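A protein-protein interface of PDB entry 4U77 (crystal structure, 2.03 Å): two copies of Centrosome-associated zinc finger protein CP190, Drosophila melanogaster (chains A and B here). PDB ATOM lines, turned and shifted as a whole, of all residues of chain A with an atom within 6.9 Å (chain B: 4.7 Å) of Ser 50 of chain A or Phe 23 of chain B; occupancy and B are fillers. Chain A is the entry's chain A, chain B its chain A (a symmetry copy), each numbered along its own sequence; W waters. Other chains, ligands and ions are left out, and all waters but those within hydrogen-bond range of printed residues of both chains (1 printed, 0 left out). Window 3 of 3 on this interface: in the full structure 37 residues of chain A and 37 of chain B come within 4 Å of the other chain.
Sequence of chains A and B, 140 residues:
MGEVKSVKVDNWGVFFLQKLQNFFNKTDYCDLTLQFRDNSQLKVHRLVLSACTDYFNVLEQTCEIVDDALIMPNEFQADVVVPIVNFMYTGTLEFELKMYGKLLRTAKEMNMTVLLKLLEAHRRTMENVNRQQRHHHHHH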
ATOM      1  N   HIS A  45      -9.476   9.199  15.121  1.00  0.00           N
ATOM      2  CA  HIS A  45     -10.443   8.281  15.720  1.00  0.00           C
ATOM      3  C   HIS A  45     -11.660   8.166  14.817  1.00  0.00           C
ATOM      4  O   HIS A  45     -12.325   9.176  14.552  1.00  0.00           O
ATOM      5  CB  HIS A  45     -10.861   8.761  17.112  1.00  0.00           C
ATOM      6  CG  HIS A  45      -9.705   9.060  18.019  1.00  0.00           C
ATOM      7  ND1 HIS A  45      -9.249  10.342  18.244  1.00  0.00           N
ATOM      8  CD2 HIS A  45      -8.906   8.243  18.747  1.00  0.00           C
ATOM      9  CE1 HIS A  45      -8.221  10.301  19.076  1.00  0.00           C
ATOM     10  NE2 HIS A  45      -7.996   9.041  19.401  1.00  0.00           N
ATOM     11  N   ARG A  46     -11.942   6.947  14.349  1.00  0.00           N
ATOM     12  CA  ARG A  46     -13.073   6.674  13.457  1.00  0.00           C
ATOM     13  C   ARG A  46     -14.374   7.239  13.999  1.00  0.00           C
ATOM     14  O   ARG A  46     -15.217   7.751  13.254  1.00  0.00           O
ATOM     15  CB  ARG A  46     -13.244   5.166  13.244  1.00  0.00           C
ATOM     16  CG  ARG A  46     -12.070   4.489  12.565  1.00  0.00           C
ATOM     17  CD  ARG A  46     -12.306   2.990  12.432  1.00  0.00           C
ATOM     18  NE  ARG A  46     -11.177   2.305  11.805  1.00  0.00           N
ATOM     19  CZ  ARG A  46     -11.261   1.588  10.688  1.00  0.00           C
ATOM     20  NH1 ARG A  46     -12.427   1.455  10.069  1.00  0.00           N
ATOM     21  NH2 ARG A  46     -10.183   0.998  10.191  1.00  0.00           N
ATOM     22  N   LEU A  47     -14.524   7.145  15.313  1.00  0.00           N
ATOM     23  CA  LEU A  47     -15.763   7.504  15.967  1.00  0.00           C
ATOM     24  C   LEU A  47     -16.012   9.003  15.911  1.00  0.00           C
ATOM     25  O   LEU A  47     -17.151   9.444  15.744  1.00  0.00           O
ATOM     26  CB  LEU A  47     -15.735   7.023  17.416  1.00  0.00           C
ATOM     27  CG  LEU A  47     -16.994   7.277  18.231  1.00  0.00           C
ATOM     28  CD1 LEU A  47     -17.183   6.125  19.150  1.00  0.00           C
ATOM     29  CD2 LEU A  47     -16.855   8.554  19.024  1.00  0.00           C
ATOM     30  N   VAL A  48     -14.946   9.783  16.071  1.00  0.00           N
ATOM     31  CA  VAL A  48     -15.040  11.233  15.941  1.00  0.00           C
ATOM     32  C   VAL A  48     -15.461  11.571  14.510  1.00  0.00           C
ATOM     33  O   VAL A  48     -16.360  12.399  14.283  1.00  0.00           O
ATOM     34  CB  VAL A  48     -13.716  11.921  16.292  1.00  0.00           C
ATOM     35  CG1 VAL A  48     -13.756  13.403  15.910  1.00  0.00           C
ATOM     36  CG2 VAL A  48     -13.401  11.742  17.800  1.00  0.00           C
ATOM     37  N   LEU A  49     -14.837  10.895  13.552  1.00  0.00           N
ATOM     38  CA  LEU A  49     -15.169  11.111  12.149  1.00  0.00           C
ATOM     39  C   LEU A  49     -16.648  10.817  11.916  1.00  0.00           C
ATOM     40  O   LEU A  49     -17.370  11.628  11.338  1.00  0.00           O
ATOM     41  CB  LEU A  49     -14.278  10.252  11.237  1.00  0.00           C
ATOM     42  CG  LEU A  49     -13.042  11.005  10.712  1.00  0.00           C
ATOM     43  CD1 LEU A  49     -12.270  11.653  11.833  1.00  0.00           C
ATOM     44  CD2 LEU A  49     -12.124  10.080   9.919  1.00  0.00           C
ATOM     45  N   SER A  50     -17.097   9.682  12.440  1.00  0.00           N
ATOM     46  CA  SER A  50     -18.448   9.177  12.224  1.00  0.00           C
ATOM     47  C   SER A  50     -19.575  10.055  12.773  1.00  0.00           C
ATOM     48  O   SER A  50     -20.709   9.965  12.312  1.00  0.00           O
ATOM     49  CB  SER A  50     -18.565   7.779  12.835  1.00  0.00           C
ATOM     50  OG  SER A  50     -17.652   6.893  12.206  1.00  0.00           O
ATOM     51  N   ALA A  51     -19.275  10.886  13.762  1.00  0.00           N
ATOM     52  CA  ALA A  51     -20.294  11.732  14.372  1.00  0.00           C
ATOM     53  C   ALA A  51     -20.753  12.844  13.432  1.00  0.00           C
ATOM     54  O   ALA A  51     -21.872  13.347  13.556  1.00  0.00           O
ATOM     55  CB  ALA A  51     -19.771  12.332  15.667  1.00  0.00           C
ATOM     56  N   CYS A  52     -19.893  13.228  12.491  1.00  0.00           N
ATOM     57  CA  CYS A  52     -20.221  14.342  11.610  1.00  0.00           C
ATOM     58  C   CYS A  52     -20.571  13.887  10.201  1.00  0.00           C
ATOM     59  O   CYS A  52     -21.171  14.640   9.436  1.00  0.00           O
ATOM     60  CB  CYS A  52     -19.053  15.339  11.559  1.00  0.00           C
ATOM     61  SG  CYS A  52     -18.842  16.326  13.060  1.00  0.00           S
ATOM     62  N   THR A  53     -20.212  12.655   9.853  1.00  0.00           N
ATOM     63  CA  THR A  53     -20.347  12.219   8.464  1.00  0.00           C
ATOM     64  C   THR A  53     -20.281  10.717   8.356  1.00  0.00           C
ATOM     65  O   THR A  53     -19.712  10.062   9.230  1.00  0.00           O
ATOM     66  CB  THR A  53     -19.237  12.830   7.561  1.00  0.00           C
ATOM     67  OG1 THR A  53     -19.470  12.488   6.187  1.00  0.00           O
ATOM     68  CG2 THR A  53     -17.862  12.296   7.970  1.00  0.00           C
ATOM     69  N   ASP A  54     -20.876  10.171   7.288  1.00  0.00           N
ATOM     70  CA  ASP A  54     -20.678   8.756   6.939  1.00  0.00           C
ATOM     71  C   ASP A  54     -19.620   8.548   5.836  1.00  0.00           C
ATOM     72  O   ASP A  54     -19.289   7.415   5.481  1.00  0.00           O
ATOM     73  CB  ASP A  54     -21.994   8.124   6.494  1.00  0.00           C
ATOM     74  CG  ASP A  54     -23.060   8.177   7.582  1.00  0.00           C
ATOM     75  OD1 ASP A  54     -22.794   7.662   8.687  1.00  0.00           O
ATOM     76  OD2 ASP A  54     -24.164   8.713   7.322  1.00  0.00           O
ATOM     77  N   PHE A  56     -16.402   8.671   5.538  1.00  0.00           N
ATOM     78  CA  PHE A  56     -15.242   7.824   5.758  1.00  0.00           C
ATOM     79  C   PHE A  56     -15.637   6.355   5.795  1.00  0.00           C
ATOM     80  O   PHE A  56     -14.832   5.517   5.421  1.00  0.00           O
ATOM     81  CB  PHE A  56     -14.493   8.228   7.032  1.00  0.00           C
ATOM     82  CG  PHE A  56     -13.679   9.483   6.860  1.00  0.00           C
ATOM     83  CD1 PHE A  56     -14.233  10.721   7.135  1.00  0.00           C
ATOM     84  CD2 PHE A  56     -12.387   9.429   6.370  1.00  0.00           C
ATOM     85  CE1 PHE A  56     -13.508  11.877   6.954  1.00  0.00           C
ATOM     86  CE2 PHE A  56     -11.645  10.585   6.197  1.00  0.00           C
ATOM     87  CZ  PHE A  56     -12.206  11.811   6.485  1.00  0.00           C
ATOM     88  N   ASN A  57     -16.870   6.034   6.195  1.00  0.00           N
ATOM     89  CA  ASN A  57     -17.333   4.639   6.110  1.00  0.00           C
ATOM     90  C   ASN A  57     -17.307   4.150   4.667  1.00  0.00           C
ATOM     91  O   ASN A  57     -16.923   3.018   4.382  1.00  0.00           O
ATOM     92  CB  ASN A  57     -18.747   4.485   6.662  1.00  0.00           C
ATOM     93  CG  ASN A  57     -18.857   4.869   8.123  1.00  0.00           C
ATOM     94  OD1 ASN A  57     -17.876   4.844   8.870  1.00  0.00           O
ATOM     95  ND2 ASN A  57     -20.064   5.265   8.530  1.00  0.00           N
ATOM     96  N   GLU A  60     -13.503   3.578   3.431  1.00  0.00           N
ATOM     97  CA  GLU A  60     -12.873   2.312   3.835  1.00  0.00           C
ATOM     98  C   GLU A  60     -13.464   1.121   3.087  1.00  0.00           C
ATOM     99  O   GLU A  60     -12.924   0.018   3.135  1.00  0.00           O
ATOM    100  CB  GLU A  60     -13.053   2.091   5.342  1.00  0.00           C
ATOM    101  CG  GLU A  60     -12.745   3.290   6.220  1.00  0.00           C
ATOM    102  CD  GLU A  60     -13.510   3.264   7.536  1.00  0.00           C
ATOM    103  OE1 GLU A  60     -13.867   2.156   7.998  1.00  0.00           O
ATOM    104  OE2 GLU A  60     -13.761   4.352   8.105  1.00  0.00           O
ATOM    105  N   MET A  88     -13.871  18.604  13.255  1.00  0.00           N
ATOM    106  CA  MET A  88     -14.613  17.505  13.865  1.00  0.00           C
ATOM    107  C   MET A  88     -14.306  17.393  15.338  1.00  0.00           C
ATOM    108  O   MET A  88     -15.180  17.042  16.135  1.00  0.00           O
ATOM    109  CB  MET A  88     -14.312  16.184  13.162  1.00  0.00           C
ATOM    110  CG  MET A  88     -14.996  16.056  11.796  1.00  0.00           C
ATOM    111  SD  MET A  88     -14.423  14.588  10.925  1.00  0.00           S
ATOM    112  CE  MET A  88     -15.460  14.598   9.490  1.00  0.00           C
ATOM    113  N   LYS B  19     -24.339  12.803  19.679  1.00  0.00           N
ATOM    114  CA  LYS B  19     -24.061  11.826  18.625  1.00  0.00           C
ATOM    115  C   LYS B  19     -23.526  10.514  19.197  1.00  0.00           C
ATOM    116  O   LYS B  19     -23.905   9.436  18.751  1.00  0.00           O
ATOM    117  CB  LYS B  19     -23.076  12.402  17.606  1.00  0.00           C
ATOM    118  CG  LYS B  19     -23.724  12.837  16.307  1.00  0.00           C
ATOM    119  CD  LYS B  19     -24.871  13.806  16.564  1.00  0.00           C
ATOM    120  CE  LYS B  19     -25.514  14.253  15.266  1.00  0.00           C
ATOM    121  NZ  LYS B  19     -24.484  14.731  14.311  1.00  0.00           N
ATOM    122  N   LEU B  20     -22.664  10.614  20.202  1.00  0.00           N
ATOM    123  CA  LEU B  20     -22.058   9.445  20.830  1.00  0.00           C
ATOM    124  C   LEU B  20     -23.035   8.589  21.635  1.00  0.00           C
ATOM    125  O   LEU B  20     -22.954   7.356  21.621  1.00  0.00           O
ATOM    126  CB  LEU B  20     -20.916   9.888  21.739  1.00  0.00           C
ATOM    127  CG  LEU B  20     -19.601   9.359  21.182  1.00  0.00           C
ATOM    128  CD1 LEU B  20     -18.415   9.878  21.973  1.00  0.00           C
ATOM    129  CD2 LEU B  20     -19.643   7.841  21.188  1.00  0.00           C
ATOM    130  N   GLN B  21     -23.939   9.250  22.349  1.00  0.00           N
ATOM    131  CA  GLN B  21     -24.969   8.561  23.112  1.00  0.00           C
ATOM    132  C   GLN B  21     -25.881   7.776  22.175  1.00  0.00           C
ATOM    133  O   GLN B  21     -26.278   6.646  22.477  1.00  0.00           O
ATOM    134  CB  GLN B  21     -25.783   9.559  23.943  1.00  0.00           C
ATOM    135  CG  GLN B  21     -24.945  10.337  24.960  1.00  0.00           C
ATOM    136  CD  GLN B  21     -25.748  11.389  25.708  1.00  0.00           C
ATOM    137  OE1 GLN B  21     -26.967  11.484  25.549  1.00  0.00           O
ATOM    138  NE2 GLN B  21     -25.066  12.173  26.544  1.00  0.00           N
ATOM    139  N   ASN B  22     -26.209   8.389  21.040  1.00  0.00           N
ATOM    140  CA  ASN B  22     -27.058   7.747  20.042  1.00  0.00           C
ATOM    141  C   ASN B  22     -26.381   6.495  19.517  1.00  0.00           C
ATOM    142  O   ASN B  22     -26.989   5.435  19.411  1.00  0.00           O
ATOM    143  CB  ASN B  22     -27.363   8.711  18.895  1.00  0.00           C
ATOM    144  CG  ASN B  22     -28.322   8.124  17.875  1.00  0.00           C
ATOM    145  OD1 ASN B  22     -29.285   7.433  18.225  1.00  0.00           O
ATOM    146  ND2 ASN B  22     -28.055   8.390  16.598  1.00  0.00           N
ATOM    147  N   PHE B  23     -25.098   6.630  19.207  1.00  0.00           N
ATOM    148  CA  PHE B  23     -24.291   5.502  18.778  1.00  0.00           C
ATOM    149  C   PHE B  23     -24.294   4.389  19.821  1.00  0.00           C
ATOM    150  O   PHE B  23     -24.425   3.222  19.471  1.00  0.00           O
ATOM    151  CB  PHE B  23     -22.858   5.946  18.492  1.00  0.00           C
ATOM    152  CG  PHE B  23     -22.719   6.794  17.258  1.00  0.00           C
ATOM    153  CD1 PHE B  23     -23.712   6.797  16.280  1.00  0.00           C
ATOM    154  CD2 PHE B  23     -21.583   7.575  17.062  1.00  0.00           C
ATOM    155  CE1 PHE B  23     -23.581   7.572  15.140  1.00  0.00           C
ATOM    156  CE2 PHE B  23     -21.443   8.353  15.918  1.00  0.00           C
ATOM    157  CZ  PHE B  23     -22.438   8.353  14.959  1.00  0.00           C
ATOM    158  N   PHE B  24     -24.158   4.760  21.094  1.00  0.00           N
ATOM    159  CA  PHE B  24     -24.113   3.786  22.186  1.00  0.00           C
ATOM    160  C   PHE B  24     -25.438   3.066  22.313  1.00  0.00           C
ATOM    161  O   PHE B  24     -25.481   1.846  22.482  1.00  0.00           O
ATOM    162  CB  PHE B  24     -23.744   4.470  23.508  1.00  0.00           C
ATOM    163  CG  PHE B  24     -23.711   3.536  24.702  1.00  0.00           C
ATOM    164  CD1 PHE B  24     -22.881   2.430  24.717  1.00  0.00           C
ATOM    165  CD2 PHE B  24     -24.491   3.790  25.821  1.00  0.00           C
ATOM    166  CE1 PHE B  24     -22.843   1.583  25.812  1.00  0.00           C
ATOM    167  CE2 PHE B  24     -24.448   2.950  26.922  1.00  0.00           C
ATOM    168  CZ  PHE B  24     -23.622   1.846  26.915  1.00  0.00           C
ATOM    169  N   ASN B  25     -26.523   3.824  22.232  1.00  0.00           N
ATOM    170  CA  ASN B  25     -27.864   3.248  22.238  1.00  0.00           C
ATOM    171  C   ASN B  25     -28.079   2.242  21.120  1.00  0.00           C
ATOM    172  O   ASN B  25     -28.622   1.156  21.337  1.00  0.00           O
ATOM    173  CB  ASN B  25     -28.932   4.339  22.120  1.00  0.00           C
ATOM    174  CG  ASN B  25     -29.040   5.191  23.362  1.00  0.00           C
ATOM    175  OD1 ASN B  25     -28.424   4.900  24.390  1.00  0.00           O
ATOM    176  ND2 ASN B  25     -29.849   6.243  23.283  1.00  0.00           N
ATOM    177  N   LYS B  26     -27.673   2.615  19.912  1.00  0.00           N
ATOM    178  CA  LYS B  26     -27.932   1.766  18.758  1.00  0.00           C
ATOM    179  C   LYS B  26     -26.792   0.787  18.543  1.00  0.00           C
ATOM    180  O   LYS B  26     -26.837  -0.025  17.620  1.00  0.00           O
ATOM    181  CB  LYS B  26     -28.166   2.616  17.508  1.00  0.00           C
ATOM    182  CG  LYS B  26     -29.520   3.310  17.496  1.00  0.00           C
ATOM    183  CD  LYS B  26     -29.622   4.344  16.390  1.00  0.00           C
ATOM    184  CE  LYS B  26     -31.042   4.889  16.290  1.00  0.00           C
ATOM    185  NZ  LYS B  26     -31.590   5.320  17.610  1.00  0.00           N
ATOM    186  N   THR B  27     -25.787   0.859  19.420  1.00  0.00           N
ATOM    187  CA  THR B  27     -24.592   0.011  19.341  1.00  0.00           C
ATOM    188  C   THR B  27     -23.923   0.110  17.958  1.00  0.00           C
ATOM    189  O   THR B  27     -23.578  -0.902  17.340  1.00  0.00           O
ATOM    190  CB  THR B  27     -24.914  -1.468  19.658  1.00  0.00           C
ATOM    191  OG1 THR B  27     -25.571  -2.067  18.539  1.00  0.00           O
ATOM    192  CG2 THR B  27     -25.820  -1.574  20.876  1.00  0.00           C
ATOM    193  N   ASP B  28     -23.759   1.343  17.482  1.00  0.00           N
ATOM    194  CA  ASP B  28     -23.005   1.633  16.265  1.00  0.00           C
ATOM    195  C   ASP B  28     -21.561   2.004  16.621  1.00  0.00           C
ATOM    196  O   ASP B  28     -21.339   2.774  17.563  1.00  0.00           O
ATOM    197  CB  ASP B  28     -23.642   2.786  15.487  1.00  0.00           C
ATOM    198  CG  ASP B  28     -24.976   2.428  14.869  1.00  0.00           C
ATOM    199  OD1 ASP B  28     -25.293   1.222  14.740  1.00  0.00           O
ATOM    200  OD2 ASP B  28     -25.716   3.375  14.527  1.00  0.00           O
ATOM    201  N   TYR B  29     -20.606   1.464  15.859  1.00  0.00           N
ATOM    202  CA  TYR B  29     -19.168   1.747  15.991  1.00  0.00           C
ATOM    203  C   TYR B  29     -18.554   1.299  17.318  1.00  0.00           C
ATOM    204  O   TYR B  29     -17.485   1.786  17.705  1.00  0.00           O
ATOM    205  CB  TYR B  29     -18.885   3.244  15.784  1.00  0.00           C
ATOM    206  CG  TYR B  29     -19.486   3.793  14.508  1.00  0.00           C
ATOM    207  CD1 TYR B  29     -19.089   3.313  13.264  1.00  0.00           C
ATOM    208  CD2 TYR B  29     -20.445   4.797  14.547  1.00  0.00           C
ATOM    209  CE1 TYR B  29     -19.639   3.812  12.090  1.00  0.00           C
ATOM    210  CE2 TYR B  29     -21.003   5.305  13.380  1.00  0.00           C
ATOM    211  CZ  TYR B  29     -20.595   4.810  12.152  1.00  0.00           C
ATOM    212  OH  TYR B  29     -21.149   5.309  10.991  1.00  0.00           O
ATOM    213  N   HIS B  45     -17.643   1.851  23.467  1.00  0.00           N
ATOM    214  CA  HIS B  45     -16.533   2.458  22.733  1.00  0.00           C
ATOM    215  C   HIS B  45     -15.350   2.645  23.667  1.00  0.00           C
ATOM    216  O   HIS B  45     -15.469   3.351  24.676  1.00  0.00           O
ATOM    217  CB  HIS B  45     -16.950   3.803  22.132  1.00  0.00           C
ATOM    218  CG  HIS B  45     -18.213   3.740  21.328  1.00  0.00           C
ATOM    219  ND1 HIS B  45     -19.435   4.135  21.830  1.00  0.00           N
ATOM    220  CD2 HIS B  45     -18.446   3.316  20.062  1.00  0.00           C
ATOM    221  CE1 HIS B  45     -20.366   3.963  20.905  1.00  0.00           C
ATOM    222  NE2 HIS B  45     -19.790   3.472  19.821  1.00  0.00           N
HETATM  223  O   HOH W   1     -22.297   8.224  11.063  1.00  0.00           O
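Of chain B, only Phe 23 (3.5 Å) and Tyr 29 (3.5 Å) come within 4 Å of Ser 50 of chain A.
Phe 23 of chain B touches just these residues of chain A: Ser 50 and Ala 51.
Of the printed residues of chain A, His 45 of chain B touches Leu 47.
Of the printed residues of chain B, Ala 51 of chain A touches Lys 19 (3.1 Å) and Phe 23 (3.9 Å).
Printed residues of chain A within 4 Å of Leu 20 of chain B: Leu 47.
Of the printed residues of chain B, Leu 47 of chain A touches Leu 20 and His 45.
Of the printed residues of chain A, Tyr 29 of chain B touches Ser 50 (3.5 Å), Asp 54 (3.7 Å) and Asn 57 (2.7 Å).
The nearest printed residue of chain B that does not touch Asn 57 of chain A is Phe 23 of chain B (7.5 Å).
N of Asp 28 of chain B lies within hydrogen-bond range of O of Phe 23 of chain B, 2.8 Å away.
A ring nitrogen (NE2) of His 45 of chain B sits at hydrogen-bond distance from the backbone carbonyl oxygen (O) of Asp 28 of chain B.
O of Arg 46 of chain A lies within hydrogen-bond range of OG of Ser 50 of chain A.
Leu 20 of chain B touches Leu 47 of chain A.
CD1 of Leu 47 of chain A touches CD2 of His 45 of chain B, at 3.2 Å.
Ser 50 of chain A touches Phe 23 of chain B (O to CZ, 3.5 Å).
Ser 50 of chain A touches Tyr 29 of chain B (CB to CE2, 3.5 Å).
Ala 51 of chain A touches Phe 23 of chain B.
Tyr 29 of chain B touches Asp 54 of chain A (OH to OD1, 3.7 Å).
Among the printed residues, 8 pairs touch across the chains.
Among the printed residues, no Asp or Glu carboxylate lies within 4 Å of a Lys or Arg side-chain nitrogen of the other chain.
The side-chain amide nitrogen (ND2) of Asn 57 of chain A is in hydrogen-bond range of the side-chain hydroxyl (OH) of Tyr 29 of chain B (2.7 Å).
The side-chain amino group of Lys 19 of chain B sits at hydrogen-bond distance from the backbone carbonyl oxygen of Ala 51 of chain A, 3.1 Å away.
Position printed for both chains: 45.
Of the 8 pairs that touch across the chains among the printed residues, none has its exchanged pair printed and touching as well.
Water W1 lies within hydrogen-bond range of OD1 of Asp 54 of chain A (2.5 Å), O of Ser 50 of chain A (2.7 Å) and OH of Tyr 29 of chain B (3.1 Å).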
